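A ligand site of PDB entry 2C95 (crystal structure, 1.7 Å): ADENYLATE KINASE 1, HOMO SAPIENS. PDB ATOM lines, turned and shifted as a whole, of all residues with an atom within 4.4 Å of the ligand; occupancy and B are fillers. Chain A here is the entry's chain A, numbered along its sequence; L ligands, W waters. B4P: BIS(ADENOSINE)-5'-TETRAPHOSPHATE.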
ATOM      1  N   GLY A  17     -27.411   5.044   3.435  1.00  0.00           N
ATOM      2  CA  GLY A  17     -26.277   5.065   4.366  1.00  0.00           C
ATOM      3  C   GLY A  17     -25.126   5.947   3.939  1.00  0.00           C
ATOM      4  O   GLY A  17     -25.102   6.498   2.825  1.00  0.00           O
ATOM      5  N   PRO A  18     -24.137   6.114   4.833  1.00  0.00           N
ATOM      6  CA  PRO A  18     -22.998   6.927   4.400  1.00  0.00           C
ATOM      7  C   PRO A  18     -22.139   6.225   3.355  1.00  0.00           C
ATOM      8  O   PRO A  18     -21.720   5.101   3.563  1.00  0.00           O
ATOM      9  CB  PRO A  18     -22.187   7.086   5.676  1.00  0.00           C
ATOM     10  CG  PRO A  18     -22.515   5.894   6.457  1.00  0.00           C
ATOM     11  CD  PRO A  18     -23.961   5.601   6.201  1.00  0.00           C
ATOM     12  N   GLY A  19     -21.860   6.884   2.243  1.00  0.00           N
ATOM     13  CA  GLY A  19     -21.186   6.203   1.143  1.00  0.00           C
ATOM     14  C   GLY A  19     -22.116   5.348   0.301  1.00  0.00           C
ATOM     15  O   GLY A  19     -21.649   4.601  -0.524  1.00  0.00           O
ATOM     16  N   SER A  20     -23.435   5.472   0.487  1.00  0.00           N
ATOM     17  CA  SER A  20     -24.416   4.710  -0.312  1.00  0.00           C
ATOM     18  C   SER A  20     -24.441   5.207  -1.765  1.00  0.00           C
ATOM     19  O   SER A  20     -24.946   4.544  -2.656  1.00  0.00           O
ATOM     20  CB  SER A  20     -25.838   4.818   0.265  1.00  0.00           C
ATOM     21  OG  SER A  20     -26.336   6.173   0.255  1.00  0.00           O
ATOM     22  N   GLY A  21     -23.895   6.387  -1.992  1.00  0.00           N
ATOM     23  CA  GLY A  21     -24.023   7.032  -3.300  1.00  0.00           C
ATOM     24  C   GLY A  21     -25.254   7.927  -3.455  1.00  0.00           C
ATOM     25  O   GLY A  21     -25.536   8.398  -4.551  1.00  0.00           O
ATOM     26  N   LYS A  22     -25.954   8.191  -2.362  1.00  0.00           N
ATOM     27  CA  LYS A  22     -27.144   9.077  -2.398  1.00  0.00           C
ATOM     28  C   LYS A  22     -26.892  10.446  -3.023  1.00  0.00           C
ATOM     29  O   LYS A  22     -27.674  10.894  -3.861  1.00  0.00           O
ATOM     30  CB  LYS A  22     -27.785   9.241  -1.003  1.00  0.00           C
ATOM     31  CG  LYS A  22     -26.916   9.881   0.056  1.00  0.00           C
ATOM     32  CD  LYS A  22     -27.537   9.905   1.445  1.00  0.00           C
ATOM     33  CE  LYS A  22     -26.645  10.725   2.412  1.00  0.00           C
ATOM     34  NZ  LYS A  22     -26.062  11.921   1.689  1.00  0.00           N
ATOM     35  N   GLY A  23     -25.777  11.092  -2.661  1.00  0.00           N
ATOM     36  CA  GLY A  23     -25.444  12.406  -3.210  1.00  0.00           C
ATOM     37  C   GLY A  23     -25.110  12.385  -4.683  1.00  0.00           C
ATOM     38  O   GLY A  23     -25.559  13.223  -5.452  1.00  0.00           O
ATOM     39  N   THR A  24     -24.284  11.415  -5.072  1.00  0.00           N
ATOM     40  CA  THR A  24     -23.953  11.164  -6.455  1.00  0.00           C
ATOM     41  C   THR A  24     -25.207  10.999  -7.325  1.00  0.00           C
ATOM     42  O   THR A  24     -25.320  11.605  -8.409  1.00  0.00           O
ATOM     43  CB  THR A  24     -23.083   9.874  -6.517  1.00  0.00           C
ATOM     44  OG1 THR A  24     -22.018  10.004  -5.571  1.00  0.00           O
ATOM     45  CG2 THR A  24     -22.522   9.621  -7.929  1.00  0.00           C
ATOM     46  N   SER A  39     -28.791  19.304   0.323  1.00  0.00           N
ATOM     47  CA  SER A  39     -28.157  18.322   1.194  1.00  0.00           C
ATOM     48  C   SER A  39     -27.922  18.925   2.584  1.00  0.00           C
ATOM     49  O   SER A  39     -27.270  19.934   2.686  1.00  0.00           O
ATOM     50  CB  SER A  39     -26.839  17.853   0.570  1.00  0.00           C
ATOM     51  OG  SER A  39     -25.954  17.396   1.595  1.00  0.00           O
ATOM     52  N   THR A  40     -28.460  18.320   3.635  1.00  0.00           N
ATOM     53  CA  THR A  40     -28.297  18.851   4.995  1.00  0.00           C
ATOM     54  C   THR A  40     -26.808  18.842   5.391  1.00  0.00           C
ATOM     55  O   THR A  40     -26.309  19.798   6.005  1.00  0.00           O
ATOM     56  CB  THR A  40     -29.232  18.123   6.046  1.00  0.00           C
ATOM     57  OG1 THR A  40     -29.228  16.700   5.816  1.00  0.00           O
ATOM     58  CG2 THR A  40     -30.678  18.660   5.955  1.00  0.00           C
ATOM     59  N   GLY A  41     -26.099  17.790   5.005  1.00  0.00           N
ATOM     60  CA  GLY A  41     -24.655  17.752   5.203  1.00  0.00           C
ATOM     61  C   GLY A  41     -23.899  18.877   4.541  1.00  0.00           C
ATOM     62  O   GLY A  41     -22.987  19.428   5.139  1.00  0.00           O
ATOM     63  N   ASP A  42     -24.259  19.197   3.300  1.00  0.00           N
ATOM     64  CA  ASP A  42     -23.652  20.344   2.612  1.00  0.00           C
ATOM     65  C   ASP A  42     -23.919  21.652   3.359  1.00  0.00           C
ATOM     66  O   ASP A  42     -23.023  22.479   3.552  1.00  0.00           O
ATOM     67  CB  ASP A  42     -24.168  20.500   1.170  1.00  0.00           C
ATOM     68  CG  ASP A  42     -23.345  19.719   0.156  1.00  0.00           C
ATOM     69  OD1 ASP A  42     -22.121  19.506   0.345  1.00  0.00           O
ATOM     70  OD2 ASP A  42     -23.942  19.358  -0.895  1.00  0.00           O
ATOM     71  N   LEU A  44     -24.630  21.999   6.597  1.00  0.00           N
ATOM     72  CA  LEU A  44     -23.821  21.937   7.830  1.00  0.00           C
ATOM     73  C   LEU A  44     -22.328  22.200   7.591  1.00  0.00           C
ATOM     74  O   LEU A  44     -21.696  22.951   8.321  1.00  0.00           O
ATOM     75  CB  LEU A  44     -24.027  20.598   8.550  1.00  0.00           C
ATOM     76  CG  LEU A  44     -25.461  20.243   9.038  1.00  0.00           C
ATOM     77  CD1 LEU A  44     -25.584  18.779   9.297  1.00  0.00           C
ATOM     78  CD2 LEU A  44     -25.919  21.063  10.266  1.00  0.00           C
ATOM     79  N   ARG A  45     -21.769  21.618   6.538  1.00  0.00           N
ATOM     80  CA  ARG A  45     -20.369  21.869   6.217  1.00  0.00           C
ATOM     81  C   ARG A  45     -20.054  23.321   5.812  1.00  0.00           C
ATOM     82  O   ARG A  45     -18.967  23.810   6.116  1.00  0.00           O
ATOM     83  CB  ARG A  45     -19.877  20.880   5.156  1.00  0.00           C
ATOM     84  CG  ARG A  45     -19.697  19.470   5.718  1.00  0.00           C
ATOM     85  CD  ARG A  45     -18.993  18.556   4.725  1.00  0.00           C
ATOM     86  NE  ARG A  45     -19.821  18.320   3.541  1.00  0.00           N
ATOM     87  CZ  ARG A  45     -20.741  17.359   3.431  1.00  0.00           C
ATOM     88  NH1 ARG A  45     -20.977  16.517   4.425  1.00  0.00           N
ATOM     89  NH2 ARG A  45     -21.434  17.252   2.297  1.00  0.00           N
ATOM     90  N   MET A  62     -20.156  16.135  13.778  1.00  0.00           N
ATOM     91  CA  MET A  62     -19.959  15.382  12.531  1.00  0.00           C
ATOM     92  C   MET A  62     -18.687  14.524  12.574  1.00  0.00           C
ATOM     93  O   MET A  62     -18.676  13.404  12.039  1.00  0.00           O
ATOM     94  CB  MET A  62     -19.949  16.274  11.270  1.00  0.00           C
ATOM     95  CG  MET A  62     -21.261  17.019  11.052  1.00  0.00           C
ATOM     96  SD  MET A  62     -21.475  17.904   9.492  1.00  0.00           S
ATOM     97  CE  MET A  62     -20.527  19.349   9.845  1.00  0.00           C
ATOM     98  N   GLN A  66     -21.946  11.603  14.688  1.00  0.00           N
ATOM     99  CA  GLN A  66     -23.265  11.681  15.324  1.00  0.00           C
ATOM    100  C   GLN A  66     -24.219  12.597  14.603  1.00  0.00           C
ATOM    101  O   GLN A  66     -23.828  13.361  13.755  1.00  0.00           O
ATOM    102  CB  GLN A  66     -23.151  12.114  16.794  1.00  0.00           C
ATOM    103  CG  GLN A  66     -22.269  11.203  17.667  1.00  0.00           C
ATOM    104  CD  GLN A  66     -22.643   9.721  17.627  1.00  0.00           C
ATOM    105  OE1 GLN A  66     -23.819   9.345  17.789  1.00  0.00           O
ATOM    106  NE2 GLN A  66     -21.642   8.866  17.415  1.00  0.00           N
ATOM    107  N   LEU A  67     -25.480  12.549  14.981  1.00  0.00           N
ATOM    108  CA  LEU A  67     -26.518  13.427  14.387  1.00  0.00           C
ATOM    109  C   LEU A  67     -26.526  14.804  15.032  1.00  0.00           C
ATOM    110  O   LEU A  67     -26.591  14.923  16.248  1.00  0.00           O
ATOM    111  CB  LEU A  67     -27.914  12.794  14.505  1.00  0.00           C
ATOM    112  CG  LEU A  67     -28.156  11.540  13.665  1.00  0.00           C
ATOM    113  CD1 LEU A  67     -29.658  11.140  13.698  1.00  0.00           C
ATOM    114  CD2 LEU A  67     -27.676  11.669  12.243  1.00  0.00           C
ATOM    115  N   VAL A  68     -26.507  15.852  14.209  1.00  0.00           N
ATOM    116  CA  VAL A  68     -26.690  17.247  14.694  1.00  0.00           C
ATOM    117  C   VAL A  68     -28.126  17.367  15.286  1.00  0.00           C
ATOM    118  O   VAL A  68     -29.032  16.696  14.785  1.00  0.00           O
ATOM    119  CB  VAL A  68     -26.466  18.244  13.495  1.00  0.00           C
ATOM    120  CG1 VAL A  68     -26.761  19.649  13.919  1.00  0.00           C
ATOM    121  CG2 VAL A  68     -25.003  18.117  12.972  1.00  0.00           C
ATOM    122  N   VAL A  73     -30.759  21.479  12.284  1.00  0.00           N
ATOM    123  CA  VAL A  73     -30.756  21.017  10.899  1.00  0.00           C
ATOM    124  C   VAL A  73     -32.068  21.321  10.166  1.00  0.00           C
ATOM    125  O   VAL A  73     -32.037  21.685   9.029  1.00  0.00           O
ATOM    126  CB  VAL A  73     -30.385  19.481  10.750  1.00  0.00           C
ATOM    127  CG1 VAL A  73     -31.260  18.616  11.619  1.00  0.00           C
ATOM    128  CG2 VAL A  73     -30.456  19.022   9.284  1.00  0.00           C
ATOM    129  N   GLY A  95     -30.397  13.229   2.591  1.00  0.00           N
ATOM    130  CA  GLY A  95     -29.858  13.022   3.951  1.00  0.00           C
ATOM    131  C   GLY A  95     -30.697  13.568   5.073  1.00  0.00           C
ATOM    132  O   GLY A  95     -30.237  13.630   6.233  1.00  0.00           O
ATOM    133  N   TYR A  96     -31.926  13.952   4.771  1.00  0.00           N
ATOM    134  CA  TYR A  96     -32.953  14.222   5.810  1.00  0.00           C
ATOM    135  C   TYR A  96     -34.229  13.551   5.302  1.00  0.00           C
ATOM    136  O   TYR A  96     -34.535  13.644   4.139  1.00  0.00           O
ATOM    137  CB  TYR A  96     -33.189  15.729   5.989  1.00  0.00           C
ATOM    138  CG  TYR A  96     -34.106  16.157   7.137  1.00  0.00           C
ATOM    139  CD1 TYR A  96     -33.577  16.798   8.263  1.00  0.00           C
ATOM    140  CD2 TYR A  96     -35.491  15.972   7.067  1.00  0.00           C
ATOM    141  CE1 TYR A  96     -34.379  17.180   9.323  1.00  0.00           C
ATOM    142  CE2 TYR A  96     -36.300  16.363   8.120  1.00  0.00           C
ATOM    143  CZ  TYR A  96     -35.755  16.970   9.242  1.00  0.00           C
ATOM    144  OH  TYR A  96     -36.553  17.335  10.305  1.00  0.00           O
ATOM    145  N   ARG A  98     -33.180  11.723   8.985  1.00  0.00           N
ATOM    146  CA  ARG A  98     -32.229  10.698   9.434  1.00  0.00           C
ATOM    147  C   ARG A  98     -32.651  10.027  10.747  1.00  0.00           C
ATOM    148  O   ARG A  98     -32.003   9.111  11.205  1.00  0.00           O
ATOM    149  CB  ARG A  98     -30.798  11.290   9.531  1.00  0.00           C
ATOM    150  CG  ARG A  98     -29.927  11.060   8.302  1.00  0.00           C
ATOM    151  CD  ARG A  98     -28.619  11.825   8.440  1.00  0.00           C
ATOM    152  NE  ARG A  98     -27.466  11.125   7.865  1.00  0.00           N
ATOM    153  CZ  ARG A  98     -26.851  11.446   6.738  1.00  0.00           C
ATOM    154  NH1 ARG A  98     -25.791  10.726   6.334  1.00  0.00           N
ATOM    155  NH2 ARG A  98     -27.264  12.463   6.007  1.00  0.00           N
ATOM    156  N   GLN A 102     -37.375  13.417  12.948  1.00  0.00           N
ATOM    157  CA  GLN A 102     -37.082  14.410  11.898  1.00  0.00           C
ATOM    158  C   GLN A 102     -38.159  14.401  10.799  1.00  0.00           C
ATOM    159  O   GLN A 102     -38.489  15.435  10.254  1.00  0.00           O
ATOM    160  CB  GLN A 102     -35.694  14.171  11.288  1.00  0.00           C
ATOM    161  CG  GLN A 102     -34.526  14.718  12.114  1.00  0.00           C
ATOM    162  CD  GLN A 102     -33.171  14.469  11.446  1.00  0.00           C
ATOM    163  OE1 GLN A 102     -33.091  14.197  10.229  1.00  0.00           O
ATOM    164  NE2 GLN A 102     -32.103  14.665  12.209  1.00  0.00           N
ATOM    165  N   ARG A 129     -16.172   2.716  -0.157  1.00  0.00           N
ATOM    166  CA  ARG A 129     -16.283   4.039  -0.825  1.00  0.00           C
ATOM    167  C   ARG A 129     -15.776   5.162   0.069  1.00  0.00           C
ATOM    168  O   ARG A 129     -15.081   6.080  -0.407  1.00  0.00           O
ATOM    169  CB  ARG A 129     -17.722   4.322  -1.279  1.00  0.00           C
ATOM    170  CG  ARG A 129     -18.183   3.387  -2.396  1.00  0.00           C
ATOM    171  CD  ARG A 129     -19.689   3.376  -2.528  1.00  0.00           C
ATOM    172  NE  ARG A 129     -20.118   2.419  -3.559  1.00  0.00           N
ATOM    173  CZ  ARG A 129     -21.381   2.275  -3.955  1.00  0.00           C
ATOM    174  NH1 ARG A 129     -22.319   3.038  -3.436  1.00  0.00           N
ATOM    175  NH2 ARG A 129     -21.713   1.385  -4.909  1.00  0.00           N
ATOM    176  N   LEU A 130     -16.072   5.090   1.369  1.00  0.00           N
ATOM    177  CA  LEU A 130     -15.618   6.122   2.285  1.00  0.00           C
ATOM    178  C   LEU A 130     -14.090   6.040   2.519  1.00  0.00           C
ATOM    179  O   LEU A 130     -13.435   7.053   2.635  1.00  0.00           O
ATOM    180  CB  LEU A 130     -16.380   6.050   3.619  1.00  0.00           C
ATOM    181  CG  LEU A 130     -17.876   6.290   3.479  1.00  0.00           C
ATOM    182  CD1 LEU A 130     -18.620   6.017   4.762  1.00  0.00           C
ATOM    183  CD2 LEU A 130     -18.199   7.698   2.961  1.00  0.00           C
ATOM    184  N   ARG A 133     -12.672   7.597  -0.557  1.00  0.00           N
ATOM    185  CA  ARG A 133     -12.803   9.077  -0.526  1.00  0.00           C
ATOM    186  C   ARG A 133     -11.802   9.683   0.455  1.00  0.00           C
ATOM    187  O   ARG A 133     -11.224  10.755   0.184  1.00  0.00           O
ATOM    188  CB  ARG A 133     -14.238   9.505  -0.201  1.00  0.00           C
ATOM    189  CG  ARG A 133     -14.470  11.013  -0.427  1.00  0.00           C
ATOM    190  CD  ARG A 133     -15.923  11.424  -0.301  1.00  0.00           C
ATOM    191  NE  ARG A 133     -16.456  11.291   1.051  1.00  0.00           N
ATOM    192  CZ  ARG A 133     -17.735  11.402   1.364  1.00  0.00           C
ATOM    193  NH1 ARG A 133     -18.663  11.682   0.442  1.00  0.00           N
ATOM    194  NH2 ARG A 133     -18.118  11.249   2.639  1.00  0.00           N
ATOM    195  N   ARG A 139     -12.878  15.638   3.695  1.00  0.00           N
ATOM    196  CA  ARG A 139     -13.950  15.140   4.596  1.00  0.00           C
ATOM    197  C   ARG A 139     -13.287  14.384   5.761  1.00  0.00           C
ATOM    198  O   ARG A 139     -13.055  13.168   5.664  1.00  0.00           O
ATOM    199  CB  ARG A 139     -14.942  14.253   3.853  1.00  0.00           C
ATOM    200  CG  ARG A 139     -15.860  15.000   2.858  1.00  0.00           C
ATOM    201  CD  ARG A 139     -17.032  15.752   3.551  1.00  0.00           C
ATOM    202  NE  ARG A 139     -17.812  14.873   4.440  1.00  0.00           N
ATOM    203  CZ  ARG A 139     -18.872  14.135   4.071  1.00  0.00           C
ATOM    204  NH1 ARG A 139     -19.379  14.197   2.844  1.00  0.00           N
ATOM    205  NH2 ARG A 139     -19.441  13.342   4.952  1.00  0.00           N
ATOM    206  N   ASP A 141     -14.366  13.516   8.507  1.00  0.00           N
ATOM    207  CA  ASP A 141     -15.231  12.451   9.010  1.00  0.00           C
ATOM    208  C   ASP A 141     -15.117  11.103   8.272  1.00  0.00           C
ATOM    209  O   ASP A 141     -15.752  10.158   8.697  1.00  0.00           O
ATOM    210  CB  ASP A 141     -16.703  12.891   9.126  1.00  0.00           C
ATOM    211  CG  ASP A 141     -17.318  13.452   7.836  1.00  0.00           C
ATOM    212  OD1 ASP A 141     -16.613  13.914   6.920  1.00  0.00           O
ATOM    213  OD2 ASP A 141     -18.584  13.442   7.759  1.00  0.00           O
ATOM    214  N   ARG A 150     -20.497   6.332  12.037  1.00  0.00           N
ATOM    215  CA  ARG A 150     -21.537   6.774  11.105  1.00  0.00           C
ATOM    216  C   ARG A 150     -22.462   5.618  10.675  1.00  0.00           C
ATOM    217  O   ARG A 150     -23.684   5.805  10.623  1.00  0.00           O
ATOM    218  CB  ARG A 150     -20.924   7.454   9.877  1.00  0.00           C
ATOM    219  CG  ARG A 150     -20.258   8.787  10.198  1.00  0.00           C
ATOM    220  CD  ARG A 150     -19.210   9.152   9.160  1.00  0.00           C
ATOM    221  NE  ARG A 150     -19.753   9.344   7.826  1.00  0.00           N
ATOM    222  CZ  ARG A 150     -19.039   9.521   6.716  1.00  0.00           C
ATOM    223  NH1 ARG A 150     -17.712   9.482   6.754  1.00  0.00           N
ATOM    224  NH2 ARG A 150     -19.654   9.692   5.555  1.00  0.00           N
ATOM    225  N   GLY A 178     -22.895  -1.444  -7.612  1.00  0.00           N
ATOM    226  CA  GLY A 178     -22.612  -1.416  -9.055  1.00  0.00           C
ATOM    227  C   GLY A 178     -22.083  -0.086  -9.515  1.00  0.00           C
ATOM    228  O   GLY A 178     -21.670   0.722  -8.686  1.00  0.00           O
ATOM    229  N   SER A 179     -22.090   0.142 -10.815  1.00  0.00           N
ATOM    230  CA  SER A 179     -21.663   1.407 -11.410  1.00  0.00           C
ATOM    231  C   SER A 179     -22.692   2.494 -11.165  1.00  0.00           C
ATOM    232  O   SER A 179     -23.871   2.231 -11.033  1.00  0.00           O
ATOM    233  CB  SER A 179     -21.484   1.261 -12.923  1.00  0.00           C
ATOM    234  OG  SER A 179     -22.746   1.168 -13.557  1.00  0.00           O
ATOM    235  N   VAL A 180     -22.234   3.730 -11.202  1.00  0.00           N
ATOM    236  CA  VAL A 180     -23.123   4.882 -11.094  1.00  0.00           C
ATOM    237  C   VAL A 180     -24.220   4.826 -12.165  1.00  0.00           C
ATOM    238  O   VAL A 180     -25.371   5.065 -11.874  1.00  0.00           O
ATOM    239  CB  VAL A 180     -22.336   6.202 -11.177  1.00  0.00           C
ATOM    240  CG1 VAL A 180     -23.280   7.395 -11.264  1.00  0.00           C
ATOM    241  CG2 VAL A 180     -21.351   6.299  -9.974  1.00  0.00           C
HETATM  242  PA  B4P L   1     -23.712  13.596   4.634  1.00  0.00           P
HETATM  243  O1A B4P L   1     -23.416  15.009   4.006  1.00  0.00           O
HETATM  244  O2A B4P L   1     -25.088  12.976   4.113  1.00  0.00           O
HETATM  245  O3A B4P L   1     -22.488  12.737   4.099  1.00  0.00           O
HETATM  246  PB  B4P L   1     -22.350  11.183   3.714  1.00  0.00           P
HETATM  247  O1B B4P L   1     -20.783  10.857   3.424  1.00  0.00           O
HETATM  248  O2B B4P L   1     -23.235  10.275   4.696  1.00  0.00           O
HETATM  249  O3B B4P L   1     -22.954  11.048   2.267  1.00  0.00           O
HETATM  250  PG  B4P L   1     -22.477  11.787   0.944  1.00  0.00           P
HETATM  251  O1G B4P L   1     -21.359  12.943   1.071  1.00  0.00           O
HETATM  252  O2G B4P L   1     -23.785  12.241   0.181  1.00  0.00           O
HETATM  253  O3G B4P L   1     -21.768  10.599   0.123  1.00  0.00           O
HETATM  254  PD  B4P L   1     -22.392   9.500  -0.930  1.00  0.00           P
HETATM  255  O1D B4P L   1     -23.049  10.302  -2.150  1.00  0.00           O
HETATM  256  O2D B4P L   1     -23.258   8.433  -0.103  1.00  0.00           O
HETATM  257  O5E B4P L   1     -23.675  13.611   6.262  1.00  0.00           O
HETATM  258  C5E B4P L   1     -22.501  14.040   6.942  1.00  0.00           C
HETATM  259  C4E B4P L   1     -22.824  14.265   8.416  1.00  0.00           C
HETATM  260  O4E B4P L   1     -23.686  15.396   8.552  1.00  0.00           O
HETATM  261  C3E B4P L   1     -23.616  13.169   9.123  1.00  0.00           C
HETATM  262  O3E B4P L   1     -22.790  12.048   9.462  1.00  0.00           O
HETATM  263  C2E B4P L   1     -24.104  13.955  10.327  1.00  0.00           C
HETATM  264  O2E B4P L   1     -23.131  14.156  11.342  1.00  0.00           O
HETATM  265  C1E B4P L   1     -24.548  15.285   9.650  1.00  0.00           C
HETATM  266  N9A B4P L   1     -25.936  15.295   9.145  1.00  0.00           N
HETATM  267  C8A B4P L   1     -26.312  15.298   7.838  1.00  0.00           C
HETATM  268  N7A B4P L   1     -27.619  15.270   7.662  1.00  0.00           N
HETATM  269  C5A B4P L   1     -28.124  15.253   8.956  1.00  0.00           C
HETATM  270  C6A B4P L   1     -29.414  15.229   9.482  1.00  0.00           C
HETATM  271  N6A B4P L   1     -30.572  15.200   8.682  1.00  0.00           N
HETATM  272  N1A B4P L   1     -29.548  15.247  10.850  1.00  0.00           N
HETATM  273  C2A B4P L   1     -28.443  15.289  11.613  1.00  0.00           C
HETATM  274  N3A B4P L   1     -27.169  15.277  11.215  1.00  0.00           N
HETATM  275  C4A B4P L   1     -27.053  15.286   9.883  1.00  0.00           C
HETATM  276  O5F B4P L   1     -21.060   8.742  -1.447  1.00  0.00           O
HETATM  277  C5F B4P L   1     -20.080   9.498  -2.079  1.00  0.00           C
HETATM  278  C4F B4P L   1     -18.869   8.639  -2.303  1.00  0.00           C
HETATM  279  O4F B4P L   1     -19.168   7.383  -2.911  1.00  0.00           O
HETATM  280  C3F B4P L   1     -17.960   9.352  -3.309  1.00  0.00           C
HETATM  281  O3F B4P L   1     -16.610   9.072  -2.986  1.00  0.00           O
HETATM  282  C2F B4P L   1     -18.467   8.813  -4.607  1.00  0.00           C
HETATM  283  O2F B4P L   1     -17.484   8.919  -5.698  1.00  0.00           O
HETATM  284  C1F B4P L   1     -18.628   7.348  -4.275  1.00  0.00           C
HETATM  285  N9B B4P L   1     -19.619   6.643  -5.112  1.00  0.00           N
HETATM  286  C8B B4P L   1     -20.931   7.003  -5.349  1.00  0.00           C
HETATM  287  N7B B4P L   1     -21.549   6.134  -6.133  1.00  0.00           N
HETATM  288  C5B B4P L   1     -20.617   5.126  -6.396  1.00  0.00           C
HETATM  289  C6B B4P L   1     -20.665   3.923  -7.116  1.00  0.00           C
HETATM  290  N6B B4P L   1     -21.804   3.470  -7.768  1.00  0.00           N
HETATM  291  N1B B4P L   1     -19.538   3.154  -7.164  1.00  0.00           N
HETATM  292  C2B B4P L   1     -18.431   3.589  -6.516  1.00  0.00           C
HETATM  293  N3B B4P L   1     -18.294   4.697  -5.788  1.00  0.00           N
HETATM  294  C4B B4P L   1     -19.403   5.438  -5.752  1.00  0.00           C
HETATM  295  O   HOH W   1     -15.551   4.828  -4.860  1.00  0.00           O
HETATM  296  O   HOH W   2     -23.849  15.948   1.568  1.00  0.00           O
HETATM  297  O   HOH W   3     -21.756  12.560  -2.997  1.00  0.00           O
HETATM  298  O   HOH W   4     -22.560  10.122   7.480  1.00  0.00           O
HETATM  299  O   HOH W   5     -21.042  14.750  -0.712  1.00  0.00           O
HETATM  300  O   HOH W   6     -24.034  10.348  11.305  1.00  0.00           O
HETATM  301  O   HOH W   7     -24.644  14.463  -0.636  1.00  0.00           O
HETATM  302  O   HOH W   8     -18.289   7.821  -8.220  1.00  0.00           O
HETATM  303  O   HOH W   9     -15.260   6.879  -3.087  1.00  0.00           O
HETATM  304  O   HOH W  10     -19.401   0.136  -6.852  1.00  0.00           O
HETATM  305  O   HOH W  11     -17.836   0.791  -4.503  1.00  0.00           O
HETATM  306  O   HOH W  12     -15.191  11.236  -4.119  1.00  0.00           O
HETATM  307  O   HOH W  13     -20.070  12.537   9.867  1.00  0.00           O
HETATM  308  O   HOH W  14     -19.764  16.139   7.095  1.00  0.00           O
HETATM  309  O   HOH W  15     -27.009  15.101   3.879  1.00  0.00           O
HETATM  310  O   HOH W  16     -24.029   5.534  -7.173  1.00  0.00           O
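An oxygen (O2E) of the ligand sits at hydrogen-bond distance from the backbone carbonyl oxygen of Gln 66, 2.6 Å away.
NH2 of Arg 150 is in salt-bridge range of O1B of the ligand (2.7 Å).
NZ of Lys 22 is in salt-bridge range of O2G of the ligand (2.7 Å).
An oxygen (O1B) of the ligand lies within salt-bridge range of the guanidinium group (NH2) of Arg 133 (2.8 Å).
The side-chain hydroxyl (OG1) of Thr 40 lies within hydrogen-bond range of a nitrogen (N7A) of the ligand, 2.8 Å away.
The backbone NH (N) of Gly 21 sits at hydrogen-bond distance from an oxygen (O2D) of the ligand, at 2.9 Å.
An oxygen (O1D) of the ligand lies within hydrogen-bond range of the backbone NH (N) of Gly 23 (2.9 Å).
NH1 of Arg 45 lies within salt-bridge range of O1A of the ligand (2.9 Å).
N6B of the ligand sits at hydrogen-bond distance from O of Gly 178 (2.9 Å).
O of Gly 95 sits at hydrogen-bond distance from N6A of the ligand (2.9 Å).
O2A of the ligand is in salt-bridge range of NH2 of Arg 98 (2.9 Å).
An oxygen (O1G) of the ligand is in salt-bridge range of the guanidinium group (NH1) of Arg 139.
The side-chain amide nitrogen of Gln 102 sits at hydrogen-bond distance from a nitrogen (N1A) of the ligand, at 3.0 Å.
O2D of the ligand sits at hydrogen-bond distance from N of Ser 20 (3.0 Å).
The backbone NH (N) of Val 68 sits at hydrogen-bond distance from a nitrogen (N3A) of the ligand, at 3.1 Å.
O2D of the ligand is in hydrogen-bond range of N of Gly 19.
The backbone NH of Thr 24 is in hydrogen-bond range of an oxygen (O1D) of the ligand, 3.4 Å away.
O of Asp 141 sits at hydrogen-bond distance from NH1 of Arg 150.
The backbone NH (N) of Lys 22 is in hydrogen-bond range of the side-chain hydroxyl (OG) of Ser 20, 3.3 Å away.
The side-chain hydroxyl (OG1) of Thr 40 lies within hydrogen-bond range of the backbone carbonyl oxygen (O) of Gly 95 (3.3 Å).
The side-chain carboxylate (OD1) of Asp 42 is in salt-bridge range of the guanidinium group (NH2) of Arg 45.
The backbone carbonyl oxygen (O) of Gly 95 is in hydrogen-bond range of the guanidinium group (NH2) of Arg 98, 3.2 Å away.
The side-chain carboxylate (OD1) of Asp 141 lies within salt-bridge range of the guanidinium group (NE) of Arg 139.
OH of Tyr 96 lies within hydrogen-bond range of O of Gln 102.
The side-chain hydroxyl (OG) of Ser 39 lies close to the backbone NH (N) of Gly 41 (3.4 Å).
The side-chain sulfur (SD) of Met 62 lies close to an oxygen (O4E) of the ligand, 3.5 Å away.
N of Val 180 lies close to N6B of the ligand.
Gly 17 touches the ligand.
Pro 18 touches the ligand.
CA of Gly 41 touches O1A of the ligand, at 3.2 Å.
Leu 44 touches the ligand (CD1 to N9A, 3.5 Å).
Leu 67 touches the ligand (CA to N3A, 3.7 Å).
CG1 of Val 73 touches N1A of the ligand, at 3.9 Å.
Tyr 96 touches the ligand (CD1 to N6A, 3.4 Å).
Arg 129 touches the ligand.
Ser 179 touches the ligand (C to N6B, 3.6 Å).
Hydrophobic or aromatic side chains within 4 Å of the ligand: Pro 18, Leu 44, Met 62, Leu 67, Val 68, Val 73, Tyr 96 and Val 180.
Of the 32 residues printed, 28 come within 4 Å of the ligand.
Water W9 lies within hydrogen-bond range of an oxygen (O3F) of the ligand (2.6 Å) and the backbone carbonyl oxygen of Arg 129 (2.8 Å).
Water W2 lies within hydrogen-bond range of OG of Ser 39 (2.6 Å), O1A of the ligand (2.6 Å) and NH2 of Arg 45 (2.8 Å).
Water W3 bridges O1D of the ligand and N of Thr 24.
Water W4 lies within hydrogen-bond range of an oxygen (O3E) of the ligand (2.8 Å), the guanidinium group (NE) of Arg 150 (2.9 Å) and the guanidinium group (NH1) of Arg 98 (3.5 Å).
Water W10 lies within hydrogen-bond range of the backbone carbonyl oxygen (O) of Gly 178, a nitrogen (N1B) of the ligand and the guanidinium group (NH2) of Arg 129.
Water W14 lies within hydrogen-bond range of the guanidinium group (NH1) of Arg 45 (3.0 Å), the side-chain carboxylate (OD2) of Asp 141 (3.0 Å) and the side-chain sulfur (SD) of Met 62 (3.4 Å).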
